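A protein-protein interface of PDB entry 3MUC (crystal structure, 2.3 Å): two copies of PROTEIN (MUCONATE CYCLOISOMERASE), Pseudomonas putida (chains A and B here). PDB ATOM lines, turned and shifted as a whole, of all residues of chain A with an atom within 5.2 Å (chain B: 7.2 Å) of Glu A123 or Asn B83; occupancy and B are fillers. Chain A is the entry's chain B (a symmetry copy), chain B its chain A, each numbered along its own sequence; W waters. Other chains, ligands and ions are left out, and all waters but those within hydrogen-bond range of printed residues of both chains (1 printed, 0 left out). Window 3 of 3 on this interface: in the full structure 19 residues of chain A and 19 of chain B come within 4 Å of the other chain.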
ATOM      1  N   LEU A 119       8.560  16.585   8.995  1.00  0.00           N
ATOM      2  CA  LEU A 119       8.381  15.935   7.695  1.00  0.00           C
ATOM      3  C   LEU A 119       6.953  15.491   7.464  1.00  0.00           C
ATOM      4  O   LEU A 119       6.233  15.218   8.419  1.00  0.00           O
ATOM      5  CB  LEU A 119       9.231  14.657   7.589  1.00  0.00           C
ATOM      6  CG  LEU A 119      10.749  14.628   7.775  1.00  0.00           C
ATOM      7  CD1 LEU A 119      11.212  13.174   7.788  1.00  0.00           C
ATOM      8  CD2 LEU A 119      11.432  15.404   6.664  1.00  0.00           C
ATOM      9  N   PRO A 120       6.519  15.455   6.194  1.00  0.00           N
ATOM     10  CA  PRO A 120       5.167  15.013   5.845  1.00  0.00           C
ATOM     11  C   PRO A 120       5.179  13.496   6.065  1.00  0.00           C
ATOM     12  O   PRO A 120       6.226  12.861   5.892  1.00  0.00           O
ATOM     13  CB  PRO A 120       5.095  15.321   4.348  1.00  0.00           C
ATOM     14  CG  PRO A 120       5.953  16.491   4.199  1.00  0.00           C
ATOM     15  CD  PRO A 120       7.153  16.116   5.040  1.00  0.00           C
ATOM     16  N   VAL A 121       4.032  12.913   6.414  1.00  0.00           N
ATOM     17  CA  VAL A 121       3.946  11.463   6.641  1.00  0.00           C
ATOM     18  C   VAL A 121       4.469  10.639   5.453  1.00  0.00           C
ATOM     19  O   VAL A 121       5.100   9.606   5.654  1.00  0.00           O
ATOM     20  CB  VAL A 121       2.500  11.019   6.970  1.00  0.00           C
ATOM     21  CG1 VAL A 121       2.373   9.497   6.968  1.00  0.00           C
ATOM     22  CG2 VAL A 121       2.100  11.538   8.316  1.00  0.00           C
ATOM     23  N   SER A 122       4.264  11.132   4.232  1.00  0.00           N
ATOM     24  CA  SER A 122       4.715  10.431   3.032  1.00  0.00           C
ATOM     25  C   SER A 122       6.229  10.254   3.024  1.00  0.00           C
ATOM     26  O   SER A 122       6.745   9.269   2.470  1.00  0.00           O
ATOM     27  CB  SER A 122       4.289  11.185   1.774  1.00  0.00           C
ATOM     28  OG  SER A 122       4.762  12.526   1.807  1.00  0.00           O
ATOM     29  N   GLU A 123       6.932  11.230   3.602  1.00  0.00           N
ATOM     30  CA  GLU A 123       8.384  11.186   3.694  1.00  0.00           C
ATOM     31  C   GLU A 123       8.805  10.241   4.795  1.00  0.00           C
ATOM     32  O   GLU A 123       9.835   9.582   4.672  1.00  0.00           O
ATOM     33  CB  GLU A 123       8.963  12.572   3.913  1.00  0.00           C
ATOM     34  CG  GLU A 123       8.513  13.597   2.879  1.00  0.00           C
ATOM     35  CD  GLU A 123       8.508  13.061   1.467  1.00  0.00           C
ATOM     36  OE1 GLU A 123       9.593  12.850   0.893  1.00  0.00           O
ATOM     37  OE2 GLU A 123       7.413  12.838   0.938  1.00  0.00           O
ATOM     38  N   LEU A 124       8.012  10.156   5.857  1.00  0.00           N
ATOM     39  CA  LEU A 124       8.297   9.213   6.942  1.00  0.00           C
ATOM     40  C   LEU A 124       8.153   7.810   6.368  1.00  0.00           C
ATOM     41  O   LEU A 124       8.859   6.892   6.768  1.00  0.00           O
ATOM     42  CB  LEU A 124       7.301   9.351   8.089  1.00  0.00           C
ATOM     43  CG  LEU A 124       7.401  10.486   9.098  1.00  0.00           C
ATOM     44  CD1 LEU A 124       6.232  10.357  10.061  1.00  0.00           C
ATOM     45  CD2 LEU A 124       8.709  10.396   9.845  1.00  0.00           C
ATOM     46  N   LEU A 125       7.223   7.658   5.432  1.00  0.00           N
ATOM     47  CA  LEU A 125       6.985   6.366   4.811  1.00  0.00           C
ATOM     48  C   LEU A 125       7.965   6.064   3.683  1.00  0.00           C
ATOM     49  O   LEU A 125       7.782   5.104   2.952  1.00  0.00           O
ATOM     50  CB  LEU A 125       5.548   6.277   4.315  1.00  0.00           C
ATOM     51  CG  LEU A 125       4.478   6.411   5.400  1.00  0.00           C
ATOM     52  CD1 LEU A 125       3.127   6.465   4.734  1.00  0.00           C
ATOM     53  CD2 LEU A 125       4.532   5.253   6.390  1.00  0.00           C
ATOM     54  N   GLY A 126       8.966   6.917   3.508  1.00  0.00           N
ATOM     55  CA  GLY A 126       9.958   6.675   2.473  1.00  0.00           C
ATOM     56  C   GLY A 126      10.227   7.759   1.446  1.00  0.00           C
ATOM     57  O   GLY A 126      11.349   7.886   0.959  1.00  0.00           O
ATOM     58  N   GLY A 127       9.196   8.502   1.075  1.00  0.00           N
ATOM     59  CA  GLY A 127       9.368   9.538   0.083  1.00  0.00           C
ATOM     60  C   GLY A 127       8.315   9.419  -0.996  1.00  0.00           C
ATOM     61  O   GLY A 127       8.064   8.331  -1.527  1.00  0.00           O
ATOM     62  N   ARG A 128       7.675  10.536  -1.308  1.00  0.00           N
ATOM     63  CA  ARG A 128       6.638  10.564  -2.333  1.00  0.00           C
ATOM     64  C   ARG A 128       7.244  10.595  -3.740  1.00  0.00           C
ATOM     65  O   ARG A 128       8.360  11.094  -3.937  1.00  0.00           O
ATOM     66  CB  ARG A 128       5.742  11.791  -2.123  1.00  0.00           C
ATOM     67  CG  ARG A 128       6.455  13.127  -2.344  1.00  0.00           C
ATOM     68  CD  ARG A 128       6.028  14.158  -1.333  1.00  0.00           C
ATOM     69  NE  ARG A 128       4.915  14.968  -1.779  1.00  0.00           N
ATOM     70  CZ  ARG A 128       3.975  15.442  -0.976  1.00  0.00           C
ATOM     71  NH1 ARG A 128       3.997  15.187   0.328  1.00  0.00           N
ATOM     72  NH2 ARG A 128       3.022  16.196  -1.482  1.00  0.00           N
ATOM     73  N   ALA B   1      19.058  19.110   0.975  1.00  0.00           N
ATOM     74  CA  ALA B   1      20.276  18.261   0.765  1.00  0.00           C
ATOM     75  C   ALA B   1      20.142  17.417  -0.489  1.00  0.00           C
ATOM     76  O   ALA B   1      19.145  16.698  -0.661  1.00  0.00           O
ATOM     77  CB  ALA B   1      20.526  17.355   1.971  1.00  0.00           C
ATOM     78  N   ILE B   3      22.371  14.897  -3.478  1.00  0.00           N
ATOM     79  CA  ILE B   3      23.470  13.961  -3.611  1.00  0.00           C
ATOM     80  C   ILE B   3      24.466  14.624  -4.546  1.00  0.00           C
ATOM     81  O   ILE B   3      24.113  14.952  -5.680  1.00  0.00           O
ATOM     82  CB  ILE B   3      22.999  12.636  -4.240  1.00  0.00           C
ATOM     83  CG1 ILE B   3      22.004  11.955  -3.303  1.00  0.00           C
ATOM     84  CG2 ILE B   3      24.189  11.727  -4.493  1.00  0.00           C
ATOM     85  CD1 ILE B   3      21.250  10.816  -3.926  1.00  0.00           C
ATOM     86  N   LEU B  79      19.725  14.530  -7.199  1.00  0.00           N
ATOM     87  CA  LEU B  79      18.441  14.216  -6.565  1.00  0.00           C
ATOM     88  C   LEU B  79      18.495  14.471  -5.084  1.00  0.00           C
ATOM     89  O   LEU B  79      19.569  14.482  -4.493  1.00  0.00           O
ATOM     90  CB  LEU B  79      18.045  12.752  -6.773  1.00  0.00           C
ATOM     91  CG  LEU B  79      17.939  12.152  -8.167  1.00  0.00           C
ATOM     92  CD1 LEU B  79      17.450  10.728  -8.020  1.00  0.00           C
ATOM     93  CD2 LEU B  79      16.995  12.954  -9.032  1.00  0.00           C
ATOM     94  N   ALA B  80      17.321  14.645  -4.484  1.00  0.00           N
ATOM     95  CA  ALA B  80      17.193  14.872  -3.046  1.00  0.00           C
ATOM     96  C   ALA B  80      17.707  13.634  -2.321  1.00  0.00           C
ATOM     97  O   ALA B  80      17.233  12.523  -2.566  1.00  0.00           O
ATOM     98  CB  ALA B  80      15.730  15.122  -2.676  1.00  0.00           C
ATOM     99  N   ALA B  81      18.679  13.845  -1.440  1.00  0.00           N
ATOM    100  CA  ALA B  81      19.291  12.778  -0.658  1.00  0.00           C
ATOM    101  C   ALA B  81      18.323  12.238   0.386  1.00  0.00           C
ATOM    102  O   ALA B  81      18.468  11.102   0.841  1.00  0.00           O
ATOM    103  CB  ALA B  81      20.549  13.297   0.018  1.00  0.00           C
ATOM    104  N   ASP B  82      17.339  13.062   0.746  1.00  0.00           N
ATOM    105  CA  ASP B  82      16.338  12.714   1.742  1.00  0.00           C
ATOM    106  C   ASP B  82      15.110  11.963   1.226  1.00  0.00           C
ATOM    107  O   ASP B  82      14.198  11.667   2.005  1.00  0.00           O
ATOM    108  CB  ASP B  82      15.911  13.962   2.504  1.00  0.00           C
ATOM    109  CG  ASP B  82      15.526  15.088   1.582  1.00  0.00           C
ATOM    110  OD1 ASP B  82      16.437  15.779   1.091  1.00  0.00           O
ATOM    111  OD2 ASP B  82      14.319  15.271   1.334  1.00  0.00           O
ATOM    112  N   ASN B  83      15.049  11.716  -0.081  1.00  0.00           N
ATOM    113  CA  ASN B  83      13.934  10.962  -0.635  1.00  0.00           C
ATOM    114  C   ASN B  83      14.510   9.647  -1.158  1.00  0.00           C
ATOM    115  O   ASN B  83      14.806   9.498  -2.351  1.00  0.00           O
ATOM    116  CB  ASN B  83      13.211  11.748  -1.729  1.00  0.00           C
ATOM    117  CG  ASN B  83      11.869  11.108  -2.124  1.00  0.00           C
ATOM    118  OD1 ASN B  83      11.688   9.885  -2.064  1.00  0.00           O
ATOM    119  ND2 ASN B  83      10.930  11.944  -2.531  1.00  0.00           N
ATOM    120  N   ILE B  84      14.679   8.695  -0.245  1.00  0.00           N
ATOM    121  CA  ILE B  84      15.264   7.397  -0.565  1.00  0.00           C
ATOM    122  C   ILE B  84      14.409   6.555  -1.498  1.00  0.00           C
ATOM    123  O   ILE B  84      14.927   5.936  -2.421  1.00  0.00           O
ATOM    124  CB  ILE B  84      15.651   6.632   0.724  1.00  0.00           C
ATOM    125  CG1 ILE B  84      16.686   7.464   1.485  1.00  0.00           C
ATOM    126  CG2 ILE B  84      16.235   5.230   0.388  1.00  0.00           C
ATOM    127  CD1 ILE B  84      16.954   6.981   2.859  1.00  0.00           C
ATOM    128  N   ASN B  85      13.097   6.590  -1.296  1.00  0.00           N
ATOM    129  CA  ASN B  85      12.150   5.848  -2.120  1.00  0.00           C
ATOM    130  C   ASN B  85      12.269   6.281  -3.602  1.00  0.00           C
ATOM    131  O   ASN B  85      12.483   5.441  -4.496  1.00  0.00           O
ATOM    132  CB  ASN B  85      10.724   6.076  -1.612  1.00  0.00           C
ATOM    133  CG  ASN B  85       9.710   5.154  -2.259  1.00  0.00           C
ATOM    134  OD1 ASN B  85       9.999   3.991  -2.539  1.00  0.00           O
ATOM    135  ND2 ASN B  85       8.523   5.661  -2.490  1.00  0.00           N
ATOM    136  N   ALA B  86      12.218   7.595  -3.837  1.00  0.00           N
ATOM    137  CA  ALA B  86      12.309   8.132  -5.195  1.00  0.00           C
ATOM    138  C   ALA B  86      13.609   7.733  -5.867  1.00  0.00           C
ATOM    139  O   ALA B  86      13.611   7.377  -7.053  1.00  0.00           O
ATOM    140  CB  ALA B  86      12.159   9.654  -5.194  1.00  0.00           C
ATOM    141  N   ALA B  87      14.703   7.768  -5.102  1.00  0.00           N
ATOM    142  CA  ALA B  87      16.028   7.412  -5.601  1.00  0.00           C
ATOM    143  C   ALA B  87      16.139   5.940  -5.977  1.00  0.00           C
ATOM    144  O   ALA B  87      16.651   5.602  -7.045  1.00  0.00           O
ATOM    145  CB  ALA B  87      17.081   7.758  -4.565  1.00  0.00           C
ATOM    146  N   MET B  88      15.633   5.066  -5.109  1.00  0.00           N
ATOM    147  CA  MET B  88      15.710   3.633  -5.341  1.00  0.00           C
ATOM    148  C   MET B  88      14.772   3.164  -6.436  1.00  0.00           C
ATOM    149  O   MET B  88      15.107   2.239  -7.181  1.00  0.00           O
ATOM    150  CB  MET B  88      15.468   2.869  -4.058  1.00  0.00           C
ATOM    151  CG  MET B  88      16.476   3.174  -2.978  1.00  0.00           C
ATOM    152  SD  MET B  88      18.209   3.192  -3.519  1.00  0.00           S
ATOM    153  CE  MET B  88      18.446   1.493  -4.034  1.00  0.00           C
ATOM    154  N   LEU B  89      13.624   3.826  -6.567  1.00  0.00           N
ATOM    155  CA  LEU B  89      12.674   3.482  -7.621  1.00  0.00           C
ATOM    156  C   LEU B  89      13.253   3.888  -8.970  1.00  0.00           C
ATOM    157  O   LEU B  89      13.040   3.200  -9.972  1.00  0.00           O
ATOM    158  CB  LEU B  89      11.321   4.164  -7.395  1.00  0.00           C
ATOM    159  CG  LEU B  89      10.383   3.455  -6.417  1.00  0.00           C
ATOM    160  CD1 LEU B  89       9.076   4.215  -6.308  1.00  0.00           C
ATOM    161  CD2 LEU B  89      10.123   2.047  -6.865  1.00  0.00           C
ATOM    162  N   LEU B 109      22.529   5.830   1.647  1.00  0.00           N
ATOM    163  CA  LEU B 109      21.513   6.879   1.731  1.00  0.00           C
ATOM    164  C   LEU B 109      20.828   6.833   3.101  1.00  0.00           C
ATOM    165  O   LEU B 109      20.546   7.874   3.703  1.00  0.00           O
ATOM    166  CB  LEU B 109      20.483   6.727   0.611  1.00  0.00           C
ATOM    167  CG  LEU B 109      20.997   6.934  -0.815  1.00  0.00           C
ATOM    168  CD1 LEU B 109      19.839   6.763  -1.801  1.00  0.00           C
ATOM    169  CD2 LEU B 109      21.638   8.317  -0.960  1.00  0.00           C
ATOM    170  N   GLN B 113      20.888   9.785   5.926  1.00  0.00           N
ATOM    171  CA  GLN B 113      19.592  10.266   6.415  1.00  0.00           C
ATOM    172  C   GLN B 113      19.432  10.082   7.938  1.00  0.00           C
ATOM    173  O   GLN B 113      18.750  10.881   8.612  1.00  0.00           O
ATOM    174  CB  GLN B 113      18.442   9.586   5.665  1.00  0.00           C
ATOM    175  CG  GLN B 113      17.037  10.071   6.043  1.00  0.00           C
ATOM    176  CD  GLN B 113      16.677  11.468   5.512  1.00  0.00           C
ATOM    177  OE1 GLN B 113      17.515  12.197   4.981  1.00  0.00           O
ATOM    178  NE2 GLN B 113      15.406  11.823   5.634  1.00  0.00           N
ATOM    179  N   ARG B 116      21.575  12.798   9.530  1.00  0.00           N
ATOM    180  CA  ARG B 116      20.885  14.051   9.258  1.00  0.00           C
ATOM    181  C   ARG B 116      19.758  14.311  10.260  1.00  0.00           C
ATOM    182  O   ARG B 116      19.642  15.419  10.792  1.00  0.00           O
ATOM    183  CB  ARG B 116      20.351  13.998   7.835  1.00  0.00           C
ATOM    184  CG  ARG B 116      19.552  15.192   7.380  1.00  0.00           C
ATOM    185  CD  ARG B 116      19.210  15.036   5.909  1.00  0.00           C
ATOM    186  NE  ARG B 116      20.398  15.072   5.044  1.00  0.00           N
ATOM    187  CZ  ARG B 116      20.785  14.101   4.218  1.00  0.00           C
ATOM    188  NH1 ARG B 116      20.083  12.978   4.113  1.00  0.00           N
ATOM    189  NH2 ARG B 116      21.891  14.250   3.496  1.00  0.00           N
ATOM    190  N   LEU B 124      14.548   4.729  11.416  1.00  0.00           N
ATOM    191  CA  LEU B 124      14.090   5.265  10.134  1.00  0.00           C
ATOM    192  C   LEU B 124      13.227   4.187   9.506  1.00  0.00           C
ATOM    193  O   LEU B 124      12.257   4.486   8.818  1.00  0.00           O
ATOM    194  CB  LEU B 124      15.254   5.542   9.183  1.00  0.00           C
ATOM    195  CG  LEU B 124      16.141   6.766   9.346  1.00  0.00           C
ATOM    196  CD1 LEU B 124      17.228   6.679   8.302  1.00  0.00           C
ATOM    197  CD2 LEU B 124      15.337   8.037   9.163  1.00  0.00           C
HETATM  198  O   HOH W   1      13.557   8.272   2.767  1.00  0.00           O
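O of Arg A128 lies within hydrogen-bond range of ND2 of Asn B83 (3.1 Å). The backbone NH (N) of Asn B85 sits at hydrogen-bond distance from the backbone carbonyl oxygen (O) of Gly A126 (3.1 Å). O of Gly A127 sits at hydrogen-bond distance from ND2 of Asn B85, at 2.9 Å.
N of Ala B86 is in hydrogen-bond range of OD1 of Asn B83, 2.9 Å away. The side-chain hydroxyl of Ser A122 lies within hydrogen-bond range of the side-chain carboxylate of Glu A123. O of Ser A122 sits at hydrogen-bond distance from N of Gly A127 (2.9 Å). The side-chain hydroxyl (OG) of Ser A122 lies within hydrogen-bond range of the guanidinium group (NH1) of Arg A128. OE2 of Glu A123 sits close to N of Arg A128, at 3.2 Å.
Among the printed residues, pairs that only touch across the chains: Glu A123 with Asn B83, Gly A126 with Asn B83, Gly A126 with Ile B84 and Gly A127 with Asn B83.
Glu A123 touches just one residue of chain B: Asn B83 (3.8 Å). Asn B83 touches four residues of chain A. Of the printed residues of chain B, Gly A126 touches Asn B83 (3.6 Å), Ile B84 (3.6 Å) and Asn B85 (3.1 Å). Of the printed residues of chain B, Gly A127 touches Asn B83 (3.2 Å) and Asn B85 (2.9 Å). Of the printed residues of chain B, Arg A128 touches Asn B83 (3.1 Å). Of the printed residues of chain A, Ile B84 touches Gly A126. Of the printed residues of chain A, Asn B85 touches Gly A126 and Gly A127. The nearest printed residue of chain A that does not touch Asn B83 is Ser A122 (6.7 Å).
Among the printed residues, 7 pairs touch across the chains. Among the printed residues, no Asp or Glu carboxylate lies within 4 Å of a Lys or Arg side-chain nitrogen of the other chain.
1 position is printed for both chains. Of the 7 pairs that touch across the chains among the printed residues, none has its exchanged pair printed and touching as well.
Water W1 bridges O of Gly A126 (2.9 Å) and N of Ile B84 (3.2 Å).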
